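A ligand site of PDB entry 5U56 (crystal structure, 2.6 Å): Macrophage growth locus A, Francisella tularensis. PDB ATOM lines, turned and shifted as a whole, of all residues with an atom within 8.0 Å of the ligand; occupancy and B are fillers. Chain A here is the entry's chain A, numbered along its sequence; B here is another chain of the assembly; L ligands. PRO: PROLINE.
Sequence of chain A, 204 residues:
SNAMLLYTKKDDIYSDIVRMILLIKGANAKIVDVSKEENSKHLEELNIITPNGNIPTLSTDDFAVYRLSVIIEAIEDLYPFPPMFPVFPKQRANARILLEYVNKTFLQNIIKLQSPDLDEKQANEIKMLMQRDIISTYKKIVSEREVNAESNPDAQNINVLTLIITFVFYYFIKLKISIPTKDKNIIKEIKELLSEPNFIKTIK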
ATOM      1  N   ASP A  12      11.433   7.574  14.382  1.00  0.00           N
ATOM      2  CA  ASP A  12      10.926   8.231  15.582  1.00  0.00           C
ATOM      3  C   ASP A  12       9.915   9.291  15.164  1.00  0.00           C
ATOM      4  O   ASP A  12      10.254  10.214  14.422  1.00  0.00           O
ATOM      5  CB  ASP A  12      12.068   8.853  16.382  1.00  0.00           C
ATOM      6  CG  ASP A  12      11.587   9.647  17.576  1.00  0.00           C
ATOM      7  OD1 ASP A  12      11.663  10.887  17.536  1.00  0.00           O
ATOM      8  OD2 ASP A  12      11.125   9.029  18.566  1.00  0.00           O
ATOM      9  N   TYR A  14       8.471  11.604  16.916  1.00  0.00           N
ATOM     10  CA  TYR A  14       8.830  12.926  17.410  1.00  0.00           C
ATOM     11  C   TYR A  14       9.870  13.586  16.519  1.00  0.00           C
ATOM     12  O   TYR A  14       9.790  14.778  16.227  1.00  0.00           O
ATOM     13  CB  TYR A  14       9.330  12.842  18.848  1.00  0.00           C
ATOM     14  CG  TYR A  14       8.280  12.481  19.870  1.00  0.00           C
ATOM     15  CD1 TYR A  14       7.432  13.442  20.384  1.00  0.00           C
ATOM     16  CD2 TYR A  14       8.150  11.173  20.327  1.00  0.00           C
ATOM     17  CE1 TYR A  14       6.475  13.115  21.326  1.00  0.00           C
ATOM     18  CE2 TYR A  14       7.199  10.844  21.262  1.00  0.00           C
ATOM     19  CZ  TYR A  14       6.365  11.813  21.757  1.00  0.00           C
ATOM     20  OH  TYR A  14       5.407  11.487  22.700  1.00  0.00           O
ATOM     21  N   SER A  15      10.860  12.803  16.084  1.00  0.00           N
ATOM     22  CA  SER A  15      11.902  13.352  15.215  1.00  0.00           C
ATOM     23  C   SER A  15      11.326  13.828  13.890  1.00  0.00           C
ATOM     24  O   SER A  15      11.746  14.857  13.357  1.00  0.00           O
ATOM     25  CB  SER A  15      12.984  12.286  14.969  1.00  0.00           C
ATOM     26  OG  SER A  15      13.682  11.991  16.167  1.00  0.00           O
ATOM     27  N   ASN A  54      18.173  11.967  25.179  1.00  0.00           N
ATOM     28  CA  ASN A  54      16.787  12.146  24.764  1.00  0.00           C
ATOM     29  C   ASN A  54      16.700  12.396  23.262  1.00  0.00           C
ATOM     30  O   ASN A  54      17.471  13.176  22.697  1.00  0.00           O
ATOM     31  CB  ASN A  54      16.164  13.312  25.526  1.00  0.00           C
ATOM     32  CG  ASN A  54      16.300  13.169  27.023  1.00  0.00           C
ATOM     33  OD1 ASN A  54      17.403  13.209  27.563  1.00  0.00           O
ATOM     34  ND2 ASN A  54      15.173  13.012  27.704  1.00  0.00           N
ATOM     35  N   ILE A  55      15.755  11.721  22.617  1.00  0.00           N
ATOM     36  CA  ILE A  55      15.499  11.880  21.187  1.00  0.00           C
ATOM     37  C   ILE A  55      14.057  12.293  20.977  1.00  0.00           C
ATOM     38  O   ILE A  55      13.137  11.632  21.474  1.00  0.00           O
ATOM     39  CB  ILE A  55      15.839  10.595  20.410  1.00  0.00           C
ATOM     40  CG1 ILE A  55      17.351  10.352  20.414  1.00  0.00           C
ATOM     41  CG2 ILE A  55      15.308  10.671  18.990  1.00  0.00           C
ATOM     42  CD1 ILE A  55      18.141  11.440  19.720  1.00  0.00           C
ATOM     43  N   PRO A  56      13.831  13.396  20.255  1.00  0.00           N
ATOM     44  CA  PRO A  56      14.893  14.211  19.670  1.00  0.00           C
ATOM     45  C   PRO A  56      15.377  15.294  20.623  1.00  0.00           C
ATOM     46  O   PRO A  56      14.753  15.524  21.665  1.00  0.00           O
ATOM     47  CB  PRO A  56      14.220  14.833  18.435  1.00  0.00           C
ATOM     48  CG  PRO A  56      12.734  14.793  18.739  1.00  0.00           C
ATOM     49  CD  PRO A  56      12.505  13.972  19.986  1.00  0.00           C
ATOM     50  N   TYR A  66      14.531  18.884  24.827  1.00  0.00           N
ATOM     51  CA  TYR A  66      14.230  17.545  24.332  1.00  0.00           C
ATOM     52  C   TYR A  66      12.775  17.087  24.425  1.00  0.00           C
ATOM     53  O   TYR A  66      12.449  16.083  23.783  1.00  0.00           O
ATOM     54  CB  TYR A  66      15.106  16.528  25.052  1.00  0.00           C
ATOM     55  CG  TYR A  66      15.308  16.779  26.527  1.00  0.00           C
ATOM     56  CD1 TYR A  66      14.367  16.377  27.465  1.00  0.00           C
ATOM     57  CD2 TYR A  66      16.456  17.413  26.993  1.00  0.00           C
ATOM     58  CE1 TYR A  66      14.554  16.603  28.815  1.00  0.00           C
ATOM     59  CE2 TYR A  66      16.655  17.644  28.338  1.00  0.00           C
ATOM     60  CZ  TYR A  66      15.704  17.234  29.244  1.00  0.00           C
ATOM     61  OH  TYR A  66      15.898  17.457  30.586  1.00  0.00           O
ATOM     62  N   ARG A  67      11.900  17.748  25.180  1.00  0.00           N
ATOM     63  CA  ARG A  67      10.506  17.325  25.221  1.00  0.00           C
ATOM     64  C   ARG A  67       9.714  18.074  24.143  1.00  0.00           C
ATOM     65  O   ARG A  67       9.948  19.262  23.903  1.00  0.00           O
ATOM     66  CB  ARG A  67       9.904  17.558  26.602  1.00  0.00           C
ATOM     67  CG  ARG A  67      10.765  16.964  27.719  1.00  0.00           C
ATOM     68  CD  ARG A  67       9.929  16.326  28.830  1.00  0.00           C
ATOM     69  NE  ARG A  67      10.780  15.720  29.847  1.00  0.00           N
ATOM     70  CZ  ARG A  67      11.224  16.341  30.932  1.00  0.00           C
ATOM     71  NH1 ARG A  67      10.900  17.614  31.150  1.00  0.00           N
ATOM     72  NH2 ARG A  67      11.991  15.700  31.810  1.00  0.00           N
ATOM     73  N   LEU A  68       8.781  17.354  23.494  1.00  0.00           N
ATOM     74  CA  LEU A  68       8.187  17.855  22.255  1.00  0.00           C
ATOM     75  C   LEU A  68       7.520  19.211  22.440  1.00  0.00           C
ATOM     76  O   LEU A  68       7.687  20.100  21.602  1.00  0.00           O
ATOM     77  CB  LEU A  68       7.166  16.844  21.713  1.00  0.00           C
ATOM     78  CG  LEU A  68       6.525  17.312  20.403  1.00  0.00           C
ATOM     79  CD1 LEU A  68       7.495  17.185  19.246  1.00  0.00           C
ATOM     80  CD2 LEU A  68       5.229  16.573  20.125  1.00  0.00           C
ATOM     81  N   SER A  69       6.759  19.376  23.519  1.00  0.00           N
ATOM     82  CA  SER A  69       6.116  20.672  23.756  1.00  0.00           C
ATOM     83  C   SER A  69       7.152  21.771  23.949  1.00  0.00           C
ATOM     84  O   SER A  69       6.953  22.905  23.508  1.00  0.00           O
ATOM     85  CB  SER A  69       5.191  20.584  24.962  1.00  0.00           C
ATOM     86  OG  SER A  69       5.908  20.282  26.138  1.00  0.00           O
ATOM     87  N   VAL A  70       8.276  21.452  24.601  1.00  0.00           N
ATOM     88  CA  VAL A  70       9.326  22.446  24.810  1.00  0.00           C
ATOM     89  C   VAL A  70      10.031  22.756  23.500  1.00  0.00           C
ATOM     90  O   VAL A  70      10.349  23.921  23.217  1.00  0.00           O
ATOM     91  CB  VAL A  70      10.308  21.968  25.886  1.00  0.00           C
ATOM     92  CG1 VAL A  70      11.236  23.101  26.300  1.00  0.00           C
ATOM     93  CG2 VAL A  70       9.554  21.419  27.093  1.00  0.00           C
ATOM     94  N   ILE A  71      10.296  21.729  22.690  1.00  0.00           N
ATOM     95  CA  ILE A  71      10.979  21.940  21.418  1.00  0.00           C
ATOM     96  C   ILE A  71      10.132  22.807  20.500  1.00  0.00           C
ATOM     97  O   ILE A  71      10.634  23.725  19.842  1.00  0.00           O
ATOM     98  CB  ILE A  71      11.326  20.585  20.763  1.00  0.00           C
ATOM     99  CG1 ILE A  71      12.390  19.859  21.581  1.00  0.00           C
ATOM    100  CG2 ILE A  71      11.794  20.789  19.326  1.00  0.00           C
ATOM    101  CD1 ILE A  71      12.864  18.571  20.945  1.00  0.00           C
ATOM    102  N   LEU A  99      -2.666  19.558  22.176  1.00  0.00           N
ATOM    103  CA  LEU A  99      -1.368  18.986  21.857  1.00  0.00           C
ATOM    104  C   LEU A  99      -0.884  18.077  22.979  1.00  0.00           C
ATOM    105  O   LEU A  99      -0.253  17.039  22.722  1.00  0.00           O
ATOM    106  CB  LEU A  99      -0.358  20.109  21.592  1.00  0.00           C
ATOM    107  CG  LEU A  99       0.970  19.787  20.901  1.00  0.00           C
ATOM    108  CD1 LEU A  99       1.471  21.013  20.163  1.00  0.00           C
ATOM    109  CD2 LEU A  99       2.027  19.306  21.894  1.00  0.00           C
ATOM    110  N   GLU A 100      -1.168  18.438  24.227  1.00  0.00           N
ATOM    111  CA  GLU A 100      -0.833  17.563  25.348  1.00  0.00           C
ATOM    112  C   GLU A 100      -1.619  16.258  25.266  1.00  0.00           C
ATOM    113  O   GLU A 100      -1.100  15.188  25.608  1.00  0.00           O
ATOM    114  CB  GLU A 100      -1.121  18.290  26.670  1.00  0.00           C
ATOM    115  CG  GLU A 100      -0.800  17.486  27.919  1.00  0.00           C
ATOM    116  CD  GLU A 100      -1.178  18.227  29.202  1.00  0.00           C
ATOM    117  OE1 GLU A 100      -2.067  19.108  29.142  1.00  0.00           O
ATOM    118  OE2 GLU A 100      -0.580  17.934  30.262  1.00  0.00           O
ATOM    119  N   ASN A 103      -0.317  13.994  22.402  1.00  0.00           N
ATOM    120  CA  ASN A 103       0.946  13.393  22.813  1.00  0.00           C
ATOM    121  C   ASN A 103       0.727  12.226  23.757  1.00  0.00           C
ATOM    122  O   ASN A 103       1.389  11.187  23.633  1.00  0.00           O
ATOM    123  CB  ASN A 103       1.852  14.447  23.446  1.00  0.00           C
ATOM    124  CG  ASN A 103       3.162  13.874  23.942  1.00  0.00           C
ATOM    125  OD1 ASN A 103       4.015  13.484  23.154  1.00  0.00           O
ATOM    126  ND2 ASN A 103       3.323  13.821  25.260  1.00  0.00           N
ATOM    127  N   LYS A 104      -0.200  12.362  24.706  1.00  0.00           N
ATOM    128  CA  LYS A 104      -0.388  11.350  25.737  1.00  0.00           C
ATOM    129  C   LYS A 104      -1.007  10.076  25.170  1.00  0.00           C
ATOM    130  O   LYS A 104      -0.582   8.969  25.524  1.00  0.00           O
ATOM    131  CB  LYS A 104      -1.245  11.914  26.871  1.00  0.00           C
ATOM    132  CG  LYS A 104      -2.178  10.922  27.551  1.00  0.00           C
ATOM    133  CD  LYS A 104      -1.471  10.059  28.578  1.00  0.00           C
ATOM    134  CE  LYS A 104      -2.465   9.178  29.334  1.00  0.00           C
ATOM    135  NZ  LYS A 104      -1.826   8.395  30.428  1.00  0.00           N
ATOM    136  N   LEU A 107       1.022   9.858  20.533  1.00  0.00           N
ATOM    137  CA  LEU A 107       2.436   9.974  20.200  1.00  0.00           C
ATOM    138  C   LEU A 107       3.284   8.992  20.993  1.00  0.00           C
ATOM    139  O   LEU A 107       4.047   8.206  20.409  1.00  0.00           O
ATOM    140  CB  LEU A 107       2.919  11.404  20.431  1.00  0.00           C
ATOM    141  CG  LEU A 107       2.332  12.470  19.497  1.00  0.00           C
ATOM    142  CD1 LEU A 107       3.086  13.773  19.619  1.00  0.00           C
ATOM    143  CD2 LEU A 107       2.337  11.978  18.054  1.00  0.00           C
ATOM    144  N   GLN A 108       3.180   9.003  22.323  1.00  0.00           N
ATOM    145  CA  GLN A 108       4.030   8.123  23.114  1.00  0.00           C
ATOM    146  C   GLN A 108       3.534   6.683  23.143  1.00  0.00           C
ATOM    147  O   GLN A 108       4.275   5.802  23.588  1.00  0.00           O
ATOM    148  CB  GLN A 108       4.177   8.663  24.537  1.00  0.00           C
ATOM    149  CG  GLN A 108       2.890   8.935  25.290  1.00  0.00           C
ATOM    150  CD  GLN A 108       3.121   9.812  26.508  1.00  0.00           C
ATOM    151  OE1 GLN A 108       4.021  10.660  26.514  1.00  0.00           O
ATOM    152  NE2 GLN A 108       2.310   9.616  27.547  1.00  0.00           N
ATOM    153  N   ILE A 111       5.300   5.285  20.154  1.00  0.00           N
ATOM    154  CA  ILE A 111       6.674   4.958  20.536  1.00  0.00           C
ATOM    155  C   ILE A 111       6.726   3.641  21.284  1.00  0.00           C
ATOM    156  O   ILE A 111       7.636   2.819  21.075  1.00  0.00           O
ATOM    157  CB  ILE A 111       7.284   6.104  21.362  1.00  0.00           C
ATOM    158  CG1 ILE A 111       7.394   7.373  20.511  1.00  0.00           C
ATOM    159  CG2 ILE A 111       8.640   5.712  21.909  1.00  0.00           C
ATOM    160  CD1 ILE A 111       8.259   7.193  19.281  1.00  0.00           C
ATOM    161  N   LYS B  66      -0.805  22.466  33.177  1.00  0.00           N
ATOM    162  CA  LYS B  66       0.387  22.929  32.472  1.00  0.00           C
ATOM    163  C   LYS B  66       0.134  24.143  31.586  1.00  0.00           C
ATOM    164  O   LYS B  66       1.104  24.735  31.111  1.00  0.00           O
ATOM    165  CB  LYS B  66       0.971  21.794  31.627  1.00  0.00           C
ATOM    166  CG  LYS B  66       1.820  20.802  32.411  1.00  0.00           C
ATOM    167  CD  LYS B  66       2.687  19.985  31.481  1.00  0.00           C
ATOM    168  CE  LYS B  66       3.707  19.166  32.250  1.00  0.00           C
ATOM    169  NZ  LYS B  66       4.627  18.433  31.340  1.00  0.00           N
ATOM    170  N   ASP B  97       8.980  22.727  32.626  1.00  0.00           N
ATOM    171  CA  ASP B  97       8.598  21.346  32.371  1.00  0.00           C
ATOM    172  C   ASP B  97       9.277  20.401  33.359  1.00  0.00           C
ATOM    173  O   ASP B  97       8.686  19.403  33.791  1.00  0.00           O
ATOM    174  CB  ASP B  97       8.941  20.961  30.938  1.00  0.00           C
ATOM    175  CG  ASP B  97       8.106  19.804  30.422  1.00  0.00           C
ATOM    176  OD1 ASP B  97       6.994  20.044  29.911  1.00  0.00           O
ATOM    177  OD2 ASP B  97       8.571  18.645  30.531  1.00  0.00           O
ATOM    178  N   ASN B 101       7.166  18.110  36.159  1.00  0.00           N
ATOM    179  CA  ASN B 101       7.214  16.667  35.949  1.00  0.00           C
ATOM    180  C   ASN B 101       8.148  15.930  36.901  1.00  0.00           C
ATOM    181  O   ASN B 101       7.956  14.720  37.116  1.00  0.00           O
ATOM    182  CB  ASN B 101       7.645  16.346  34.517  1.00  0.00           C
ATOM    183  CG  ASN B 101       6.594  16.730  33.492  1.00  0.00           C
ATOM    184  OD1 ASN B 101       5.427  16.916  33.835  1.00  0.00           O
ATOM    185  ND2 ASN B 101       6.996  16.823  32.234  1.00  0.00           N
HETATM  186  N   PRO L   1       8.877  11.716  25.454  1.00  0.00           N
HETATM  187  CA  PRO L   1       8.951  13.166  25.242  1.00  0.00           C
HETATM  188  C   PRO L   1       7.585  13.839  25.326  1.00  0.00           C
HETATM  189  O   PRO L   1       7.433  15.001  24.970  1.00  0.00           O
HETATM  190  CB  PRO L   1       9.527  13.284  23.828  1.00  0.00           C
HETATM  191  CG  PRO L   1      10.318  12.031  23.635  1.00  0.00           C
HETATM  192  CD  PRO L   1       9.564  10.962  24.381  1.00  0.00           C
HETATM  193  OXT PRO L   1       6.607  13.229  25.759  1.00  0.00           O
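An oxygen (O) of the ligand lies within hydrogen-bond range of the backbone NH of Leu 68, at 3.1 Å.
ND2 of Asn 103 is in hydrogen-bond range of OXT of the ligand (3.4 Å).
The side-chain hydroxyl (OH) of Tyr 14 lies within hydrogen-bond range of the side-chain amide oxygen (OD1) of Asn 103, 2.5 Å away.
The backbone carbonyl oxygen (O) of Asn 103 lies within hydrogen-bond range of the backbone NH (N) of Gln 108 (3.1 Å).
N of Gln 108 sits at hydrogen-bond distance from OH of Tyr 14.
The backbone NH (N) of Tyr 14 sits close to the side-chain carboxylate (OD1) of Asp 12, 3.3 Å away.
NH1 of Arg 67 is in salt-bridge range of OD2 of Asp 97 of chain B, 2.6 Å away.
Tyr 14 touches the ligand.
Ile 55 touches the ligand.
Arg 67 touches the ligand.
Gln 108 touches the ligand (OE1 to OXT, 3.7 Å).
Hydrophobic or aromatic side chains within 4 Å of the ligand: Tyr 14 and Leu 68.
Six residues have an atom within 4 Å of the ligand: Tyr 14, Ile 55, Arg 67, Leu 68, Asn 103 and Gln 108.
The nearest printed residue that does not touch the ligand is Tyr 66 of chain A (4.05 Å).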
